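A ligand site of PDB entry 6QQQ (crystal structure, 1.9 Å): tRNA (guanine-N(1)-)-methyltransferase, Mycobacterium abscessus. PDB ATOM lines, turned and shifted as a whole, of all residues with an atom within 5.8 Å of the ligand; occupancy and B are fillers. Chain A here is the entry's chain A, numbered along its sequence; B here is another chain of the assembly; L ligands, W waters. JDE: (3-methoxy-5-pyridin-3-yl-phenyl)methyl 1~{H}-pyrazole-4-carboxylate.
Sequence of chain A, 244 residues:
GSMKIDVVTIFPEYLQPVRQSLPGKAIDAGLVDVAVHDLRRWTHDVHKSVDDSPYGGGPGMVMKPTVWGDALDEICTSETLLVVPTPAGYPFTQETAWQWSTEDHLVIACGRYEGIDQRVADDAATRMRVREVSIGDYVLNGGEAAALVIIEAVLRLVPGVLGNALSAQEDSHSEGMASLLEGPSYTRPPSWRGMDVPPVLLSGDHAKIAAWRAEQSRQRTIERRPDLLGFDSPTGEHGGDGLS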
ATOM      1  N   VAL A  84      25.210 -15.802 -27.719  1.00  0.00           N
ATOM      2  CA  VAL A  84      25.428 -15.909 -26.279  1.00  0.00           C
ATOM      3  C   VAL A  84      24.404 -15.039 -25.543  1.00  0.00           C
ATOM      4  O   VAL A  84      24.557 -13.825 -25.484  1.00  0.00           O
ATOM      5  CB  VAL A  84      26.842 -15.476 -25.885  1.00  0.00           C
ATOM      6  CG1 VAL A  84      27.070 -15.692 -24.387  1.00  0.00           C
ATOM      7  CG2 VAL A  84      27.911 -16.222 -26.730  1.00  0.00           C
ATOM      8  N   PRO A  85      23.375 -15.660 -24.985  1.00  0.00           N
ATOM      9  CA  PRO A  85      22.374 -14.894 -24.222  1.00  0.00           C
ATOM     10  C   PRO A  85      22.991 -14.364 -22.933  1.00  0.00           C
ATOM     11  O   PRO A  85      23.709 -15.086 -22.257  1.00  0.00           O
ATOM     12  CB  PRO A  85      21.281 -15.925 -23.933  1.00  0.00           C
ATOM     13  CG  PRO A  85      21.486 -17.003 -24.975  1.00  0.00           C
ATOM     14  CD  PRO A  85      22.976 -17.065 -25.153  1.00  0.00           C
ATOM     15  N   THR A  86      22.734 -13.112 -22.618  1.00  0.00           N
ATOM     16  CA  THR A  86      23.279 -12.486 -21.417  1.00  0.00           C
ATOM     17  C   THR A  86      22.530 -11.192 -21.148  1.00  0.00           C
ATOM     18  O   THR A  86      22.124 -10.527 -22.088  1.00  0.00           O
ATOM     19  CB  THR A  86      24.812 -12.202 -21.532  1.00  0.00           C
ATOM     20  OG1 THR A  86      25.207 -11.290 -20.497  1.00  0.00           O
ATOM     21  CG2 THR A  86      25.195 -11.637 -22.886  1.00  0.00           C
ATOM     22  N   PRO A  87      22.353 -10.828 -19.861  1.00  0.00           N
ATOM     23  CA  PRO A  87      21.698  -9.551 -19.549  1.00  0.00           C
ATOM     24  C   PRO A  87      22.495  -8.351 -20.062  1.00  0.00           C
ATOM     25  O   PRO A  87      21.942  -7.247 -20.172  1.00  0.00           O
ATOM     26  CB  PRO A  87      21.651  -9.523 -18.014  1.00  0.00           C
ATOM     27  CG  PRO A  87      21.862 -10.934 -17.592  1.00  0.00           C
ATOM     28  CD  PRO A  87      22.714 -11.573 -18.638  1.00  0.00           C
ATOM     29  N   ALA A 109      25.234 -20.646 -26.859  1.00  0.00           N
ATOM     30  CA  ALA A 109      25.982 -20.997 -25.665  1.00  0.00           C
ATOM     31  C   ALA A 109      25.242 -20.543 -24.420  1.00  0.00           C
ATOM     32  O   ALA A 109      25.221 -19.344 -24.109  1.00  0.00           O
ATOM     33  CB  ALA A 109      27.371 -20.381 -25.711  1.00  0.00           C
ATOM     34  N   CYS A 110      24.638 -21.491 -23.689  1.00  0.00           N
ATOM     35  CA  CYS A 110      23.901 -21.140 -22.477  1.00  0.00           C
ATOM     36  C   CYS A 110      24.810 -21.064 -21.250  1.00  0.00           C
ATOM     37  O   CYS A 110      25.363 -22.078 -20.803  1.00  0.00           O
ATOM     38  CB  CYS A 110      22.780 -22.145 -22.222  1.00  0.00           C
ATOM     39  SG  CYS A 110      21.613 -22.236 -23.590  1.00  0.00           S
ATOM     40  N   GLY A 111      24.938 -19.865 -20.712  1.00  0.00           N
ATOM     41  CA  GLY A 111      25.769 -19.654 -19.545  1.00  0.00           C
ATOM     42  C   GLY A 111      24.947 -19.693 -18.289  1.00  0.00           C
ATOM     43  O   GLY A 111      23.710 -19.592 -18.332  1.00  0.00           O
ATOM     44  N   ARG A 112      25.631 -19.858 -17.163  1.00  0.00           N
ATOM     45  CA  ARG A 112      25.006 -19.869 -15.851  1.00  0.00           C
ATOM     46  C   ARG A 112      25.812 -19.043 -14.877  1.00  0.00           C
ATOM     47  O   ARG A 112      26.834 -18.440 -15.234  1.00  0.00           O
ATOM     48  CB  ARG A 112      24.858 -21.291 -15.329  1.00  0.00           C
ATOM     49  CG  ARG A 112      23.801 -22.112 -16.052  1.00  0.00           C
ATOM     50  CD  ARG A 112      22.863 -22.731 -15.048  1.00  0.00           C
ATOM     51  NE  ARG A 112      21.465 -22.424 -15.314  1.00  0.00           N
ATOM     52  CZ  ARG A 112      20.532 -22.299 -14.375  1.00  0.00           C
ATOM     53  NH1 ARG A 112      20.861 -22.436 -13.091  1.00  0.00           N
ATOM     54  NH2 ARG A 112      19.282 -22.019 -14.707  1.00  0.00           N
ATOM     55  N   TYR A 113      25.349 -19.031 -13.630  1.00  0.00           N
ATOM     56  CA  TYR A 113      25.975 -18.279 -12.539  1.00  0.00           C
ATOM     57  C   TYR A 113      26.232 -16.850 -12.973  1.00  0.00           C
ATOM     58  O   TYR A 113      25.332 -16.216 -13.534  1.00  0.00           O
ATOM     59  CB  TYR A 113      27.254 -18.962 -12.091  1.00  0.00           C
ATOM     60  CG  TYR A 113      27.093 -20.462 -11.996  1.00  0.00           C
ATOM     61  CD1 TYR A 113      25.979 -21.024 -11.369  1.00  0.00           C
ATOM     62  CD2 TYR A 113      28.040 -21.316 -12.570  1.00  0.00           C
ATOM     63  CE1 TYR A 113      25.819 -22.402 -11.299  1.00  0.00           C
ATOM     64  CE2 TYR A 113      27.883 -22.680 -12.497  1.00  0.00           C
ATOM     65  CZ  TYR A 113      26.779 -23.224 -11.867  1.00  0.00           C
ATOM     66  OH  TYR A 113      26.636 -24.590 -11.795  1.00  0.00           O
ATOM     67  N   GLU A 114      27.441 -16.348 -12.747  1.00  0.00           N
ATOM     68  CA  GLU A 114      27.751 -14.945 -13.025  1.00  0.00           C
ATOM     69  C   GLU A 114      28.037 -14.659 -14.506  1.00  0.00           C
ATOM     70  O   GLU A 114      27.795 -13.561 -14.983  1.00  0.00           O
ATOM     71  CB  GLU A 114      28.945 -14.473 -12.180  1.00  0.00           C
ATOM     72  CG  GLU A 114      29.238 -12.971 -12.251  1.00  0.00           C
ATOM     73  CD  GLU A 114      27.980 -12.087 -12.237  1.00  0.00           C
ATOM     74  OE1 GLU A 114      26.990 -12.436 -11.541  1.00  0.00           O
ATOM     75  OE2 GLU A 114      27.973 -11.032 -12.911  1.00  0.00           O
ATOM     76  N   GLY A 115      28.549 -15.642 -15.237  1.00  0.00           N
ATOM     77  CA  GLY A 115      28.779 -15.440 -16.651  1.00  0.00           C
ATOM     78  C   GLY A 115      29.878 -16.360 -17.177  1.00  0.00           C
ATOM     79  O   GLY A 115      30.325 -17.242 -16.459  1.00  0.00           O
ATOM     80  N   ILE A 116      30.307 -16.136 -18.402  1.00  0.00           N
ATOM     81  CA  ILE A 116      31.337 -16.979 -19.030  1.00  0.00           C
ATOM     82  C   ILE A 116      32.589 -16.124 -19.161  1.00  0.00           C
ATOM     83  O   ILE A 116      32.492 -14.955 -19.498  1.00  0.00           O
ATOM     84  CB  ILE A 116      30.882 -17.482 -20.404  1.00  0.00           C
ATOM     85  CG1 ILE A 116      29.566 -18.247 -20.261  1.00  0.00           C
ATOM     86  CG2 ILE A 116      31.955 -18.364 -21.053  1.00  0.00           C
ATOM     87  CD1 ILE A 116      28.979 -18.692 -21.594  1.00  0.00           C
ATOM     88  N   VAL A 133      23.584 -11.228 -26.735  1.00  0.00           N
ATOM     89  CA  VAL A 133      22.262 -10.601 -26.845  1.00  0.00           C
ATOM     90  C   VAL A 133      21.429 -10.764 -25.584  1.00  0.00           C
ATOM     91  O   VAL A 133      21.530 -11.779 -24.897  1.00  0.00           O
ATOM     92  CB  VAL A 133      21.418 -11.173 -28.028  1.00  0.00           C
ATOM     93  CG1 VAL A 133      22.050 -10.821 -29.370  1.00  0.00           C
ATOM     94  CG2 VAL A 133      21.234 -12.697 -27.906  1.00  0.00           C
ATOM     95  N   SER A 134      20.607  -9.770 -25.294  1.00  0.00           N
ATOM     96  CA  SER A 134      19.636  -9.852 -24.202  1.00  0.00           C
ATOM     97  C   SER A 134      18.241  -9.959 -24.773  1.00  0.00           C
ATOM     98  O   SER A 134      17.905  -9.249 -25.739  1.00  0.00           O
ATOM     99  CB  SER A 134      19.736  -8.633 -23.279  1.00  0.00           C
ATOM    100  OG  SER A 134      18.555  -8.498 -22.498  1.00  0.00           O
ATOM    101  N   ILE A 135      17.413 -10.831 -24.198  1.00  0.00           N
ATOM    102  CA  ILE A 135      16.045 -10.951 -24.691  1.00  0.00           C
ATOM    103  C   ILE A 135      15.104 -10.029 -23.918  1.00  0.00           C
ATOM    104  O   ILE A 135      13.911  -9.953 -24.225  1.00  0.00           O
ATOM    105  CB  ILE A 135      15.512 -12.393 -24.604  1.00  0.00           C
ATOM    106  CG1 ILE A 135      15.511 -12.904 -23.157  1.00  0.00           C
ATOM    107  CG2 ILE A 135      16.298 -13.335 -25.547  1.00  0.00           C
ATOM    108  CD1 ILE A 135      14.535 -14.070 -22.945  1.00  0.00           C
ATOM    109  N   GLY A 136      15.630  -9.311 -22.932  1.00  0.00           N
ATOM    110  CA  GLY A 136      14.807  -8.442 -22.105  1.00  0.00           C
ATOM    111  C   GLY A 136      15.512  -7.980 -20.846  1.00  0.00           C
ATOM    112  O   GLY A 136      16.490  -8.599 -20.419  1.00  0.00           O
ATOM    113  N   ASP A 137      14.994  -6.919 -20.240  1.00  0.00           N
ATOM    114  CA  ASP A 137      15.640  -6.307 -19.089  1.00  0.00           C
ATOM    115  C   ASP A 137      15.176  -6.908 -17.779  1.00  0.00           C
ATOM    116  O   ASP A 137      14.531  -6.238 -16.953  1.00  0.00           O
ATOM    117  CB  ASP A 137      15.405  -4.784 -19.075  1.00  0.00           C
ATOM    118  CG  ASP A 137      16.255  -4.072 -20.106  1.00  0.00           C
ATOM    119  OD1 ASP A 137      17.280  -4.641 -20.531  1.00  0.00           O
ATOM    120  OD2 ASP A 137      15.917  -2.925 -20.454  1.00  0.00           O
ATOM    121  N   TYR A 138      15.503  -8.174 -17.588  1.00  0.00           N
ATOM    122  CA  TYR A 138      15.258  -8.901 -16.348  1.00  0.00           C
ATOM    123  C   TYR A 138      16.409  -9.861 -16.220  1.00  0.00           C
ATOM    124  O   TYR A 138      17.182 -10.040 -17.161  1.00  0.00           O
ATOM    125  CB  TYR A 138      13.930  -9.644 -16.374  1.00  0.00           C
ATOM    126  CG  TYR A 138      13.603 -10.152 -17.756  1.00  0.00           C
ATOM    127  CD1 TYR A 138      14.232 -11.294 -18.273  1.00  0.00           C
ATOM    128  CD2 TYR A 138      12.676  -9.500 -18.558  1.00  0.00           C
ATOM    129  CE1 TYR A 138      13.942 -11.749 -19.553  1.00  0.00           C
ATOM    130  CE2 TYR A 138      12.368  -9.948 -19.826  1.00  0.00           C
ATOM    131  CZ  TYR A 138      13.002 -11.064 -20.327  1.00  0.00           C
ATOM    132  OH  TYR A 138      12.692 -11.474 -21.597  1.00  0.00           O
ATOM    133  N   VAL A 139      16.521 -10.507 -15.064  1.00  0.00           N
ATOM    134  CA  VAL A 139      17.627 -11.433 -14.853  1.00  0.00           C
ATOM    135  C   VAL A 139      17.125 -12.863 -14.673  1.00  0.00           C
ATOM    136  O   VAL A 139      16.186 -13.102 -13.914  1.00  0.00           O
ATOM    137  CB  VAL A 139      18.477 -11.030 -13.635  1.00  0.00           C
ATOM    138  CG1 VAL A 139      19.664 -11.962 -13.461  1.00  0.00           C
ATOM    139  CG2 VAL A 139      18.950  -9.584 -13.760  1.00  0.00           C
ATOM    140  N   LEU A 140      17.768 -13.810 -15.363  1.00  0.00           N
ATOM    141  CA  LEU A 140      17.445 -15.233 -15.191  1.00  0.00           C
ATOM    142  C   LEU A 140      18.639 -15.927 -14.546  1.00  0.00           C
ATOM    143  O   LEU A 140      19.702 -15.325 -14.434  1.00  0.00           O
ATOM    144  CB  LEU A 140      17.120 -15.887 -16.544  1.00  0.00           C
ATOM    145  CG  LEU A 140      16.166 -15.112 -17.461  1.00  0.00           C
ATOM    146  CD1 LEU A 140      16.053 -15.768 -18.836  1.00  0.00           C
ATOM    147  CD2 LEU A 140      14.808 -14.971 -16.813  1.00  0.00           C
ATOM    148  N   ASN A 141      18.475 -17.188 -14.153  1.00  0.00           N
ATOM    149  CA  ASN A 141      19.588 -17.948 -13.580  1.00  0.00           C
ATOM    150  C   ASN A 141      20.578 -18.434 -14.630  1.00  0.00           C
ATOM    151  O   ASN A 141      21.773 -18.610 -14.366  1.00  0.00           O
ATOM    152  CB  ASN A 141      19.053 -19.140 -12.793  1.00  0.00           C
ATOM    153  CG  ASN A 141      18.758 -18.804 -11.342  1.00  0.00           C
ATOM    154  OD1 ASN A 141      19.230 -17.791 -10.821  1.00  0.00           O
ATOM    155  ND2 ASN A 141      17.962 -19.643 -10.700  1.00  0.00           N
ATOM    156  N   GLY A 142      20.072 -18.664 -15.830  1.00  0.00           N
ATOM    157  CA  GLY A 142      20.875 -19.231 -16.899  1.00  0.00           C
ATOM    158  C   GLY A 142      20.286 -18.874 -18.254  1.00  0.00           C
ATOM    159  O   GLY A 142      19.183 -18.332 -18.342  1.00  0.00           O
ATOM    160  N   GLY A 143      21.023 -19.176 -19.312  1.00  0.00           N
ATOM    161  CA  GLY A 143      20.597 -18.756 -20.643  1.00  0.00           C
ATOM    162  C   GLY A 143      19.602 -19.670 -21.318  1.00  0.00           C
ATOM    163  O   GLY A 143      19.158 -19.392 -22.442  1.00  0.00           O
ATOM    164  N   ALA A 146      16.250 -18.228 -22.328  1.00  0.00           N
ATOM    165  CA  ALA A 146      16.499 -17.286 -23.409  1.00  0.00           C
ATOM    166  C   ALA A 146      16.738 -18.032 -24.709  1.00  0.00           C
ATOM    167  O   ALA A 146      16.305 -17.572 -25.765  1.00  0.00           O
ATOM    168  CB  ALA A 146      17.698 -16.387 -23.076  1.00  0.00           C
ATOM    169  N   ARG B 156      13.432 -16.705  -8.659  1.00  0.00           N
ATOM    170  CA  ARG B 156      14.765 -16.529  -8.090  1.00  0.00           C
ATOM    171  C   ARG B 156      14.830 -15.333  -7.129  1.00  0.00           C
ATOM    172  O   ARG B 156      15.846 -15.123  -6.463  1.00  0.00           O
ATOM    173  CB  ARG B 156      15.809 -16.390  -9.193  1.00  0.00           C
ATOM    174  CG  ARG B 156      15.685 -15.147 -10.045  1.00  0.00           C
ATOM    175  CD  ARG B 156      16.712 -15.155 -11.169  1.00  0.00           C
ATOM    176  NE  ARG B 156      18.081 -14.984 -10.675  1.00  0.00           N
ATOM    177  CZ  ARG B 156      18.605 -13.812 -10.329  1.00  0.00           C
ATOM    178  NH1 ARG B 156      17.871 -12.704 -10.377  1.00  0.00           N
ATOM    179  NH2 ARG B 156      19.850 -13.752  -9.903  1.00  0.00           N
ATOM    180  N   GLU B 182      26.550  -5.292 -16.686  1.00  0.00           N
ATOM    181  CA  GLU B 182      27.688  -5.958 -16.063  1.00  0.00           C
ATOM    182  C   GLU B 182      28.851  -6.000 -17.058  1.00  0.00           C
ATOM    183  O   GLU B 182      28.635  -6.207 -18.259  1.00  0.00           O
ATOM    184  CB  GLU B 182      27.317  -7.383 -15.622  1.00  0.00           C
ATOM    185  CG  GLU B 182      26.389  -7.491 -14.406  1.00  0.00           C
ATOM    186  CD  GLU B 182      26.020  -8.941 -14.063  1.00  0.00           C
ATOM    187  OE1 GLU B 182      25.740  -9.715 -15.013  1.00  0.00           O
ATOM    188  OE2 GLU B 182      25.968  -9.311 -12.869  1.00  0.00           O
HETATM  189  C10 JDE L   1      18.391 -11.712 -19.484  1.00  0.00           C
HETATM  190  N12 JDE L   1      18.475 -11.822 -21.684  1.00  0.00           N
HETATM  191  C13 JDE L   1      19.165 -12.859 -21.198  1.00  0.00           C
HETATM  192  C15 JDE L   1      22.557 -14.591 -16.616  1.00  0.00           C
HETATM  193  C17 JDE L   1      23.612 -13.507 -14.648  1.00  0.00           C
HETATM  194  C20 JDE L   1      23.572 -12.376 -12.148  1.00  0.00           C
HETATM  195  C21 JDE L   1      22.647 -13.391 -12.428  1.00  0.00           C
HETATM  196  C22 JDE L   1      22.655 -13.969 -13.711  1.00  0.00           C
HETATM  197  C01 JDE L   1      26.313 -15.732 -19.774  1.00  0.00           C
HETATM  198  O02 JDE L   1      26.112 -14.706 -18.763  1.00  0.00           O
HETATM  199  C03 JDE L   1      24.909 -14.698 -18.101  1.00  0.00           C
HETATM  200  C04 JDE L   1      23.801 -15.193 -18.658  1.00  0.00           C
HETATM  201  C05 JDE L   1      22.581 -15.135 -17.933  1.00  0.00           C
HETATM  202  C06 JDE L   1      21.303 -15.668 -18.490  1.00  0.00           C
HETATM  203  O07 JDE L   1      20.713 -14.730 -19.392  1.00  0.00           O
HETATM  204  C08 JDE L   1      19.779 -13.770 -18.847  1.00  0.00           C
HETATM  205  C09 JDE L   1      19.120 -12.779 -19.805  1.00  0.00           C
HETATM  206  N11 JDE L   1      18.023 -11.138 -20.651  1.00  0.00           N
HETATM  207  O14 JDE L   1      19.533 -13.698 -17.609  1.00  0.00           O
HETATM  208  C16 JDE L   1      23.670 -14.103 -16.060  1.00  0.00           C
HETATM  209  C18 JDE L   1      24.494 -12.496 -14.274  1.00  0.00           C
HETATM  210  N19 JDE L   1      24.452 -11.966 -13.051  1.00  0.00           N
HETATM  211  C23 JDE L   1      24.867 -14.129 -16.777  1.00  0.00           C
HETATM  212  O   HOH W   1      27.377 -11.585 -19.144  1.00  0.00           O
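A nitrogen (N11) of the ligand sits at hydrogen-bond distance from the side-chain hydroxyl of Ser 134 (3.3 Å).
O of Gly 136 lies close to N11 of the ligand (3.0 Å).
O14 of the ligand lies within hydrogen-bond range of N of Leu 140 (2.9 Å).
A nitrogen (N12) of the ligand sits close to the backbone NH (N) of Ile 135 (2.9 Å).
OD1 of Asn 141 is in hydrogen-bond range of NE of Arg 156 of chain B (3.0 Å).
The backbone carbonyl oxygen (O) of Ile 135 sits at hydrogen-bond distance from the side-chain hydroxyl (OH) of Tyr 138 (3.3 Å).
OE2 of Glu 114 sits close to OE2 of Glu 182 of chain B, 2.6 Å away.
N of Thr 86 lies within hydrogen-bond range of O of Val 133 (2.9 Å).
The side-chain hydroxyl (OG) of Ser 134 sits at hydrogen-bond distance from the backbone carbonyl oxygen (O) of Gly 136 (2.9 Å).
O of Gly 111 sits at hydrogen-bond distance from N of Gly 143 (2.9 Å).
A nitrogen (N19) of the ligand lies close to the side-chain carboxylate (OE1) of Glu 114, at 3.0 Å.
A nitrogen (N19) of the ligand sits close to the side-chain carboxylate of Glu 182 of chain B (3.1 Å).
Pro 85 touches the ligand (O to C04, 3.6 Å).
Thr 86 touches the ligand (C to C13, 3.8 Å).
CG of Pro 87 touches O14 of the ligand (3.6 Å).
Gly 111 touches the ligand (CA to C01, 3.97 Å).
O of Tyr 113 touches C17 of the ligand, 3.4 Å away.
Gly 115 touches the ligand.
O of Tyr 138 touches C10 of the ligand (3.1 Å).
Val 139 touches the ligand.
Gly 142 touches the ligand (C to C06, 3.4 Å).
Gly 143 touches the ligand.
NH2 of Arg 156 of chain B touches C21 of the ligand (3.8 Å).
Hydrophobic or aromatic side chains that line the ligand: Pro 87, Ile 135, Val 139 and Leu 140.
Within 4 Å of the ligand: Pro 85, Thr 86, Pro 87, Gly 111, Tyr 113, Glu 114, Gly 115, Ser 134, Ile 135, Gly 136, Tyr 138, Val 139, Leu 140, Gly 142, Gly 143, Arg 156 of chain B and Glu 182 of chain B.
The nearest printed residue that does not touch the ligand is Ile 116 (4.1 Å).
Water W1 bridges OG1 of Thr 86 and O02 of the ligand.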
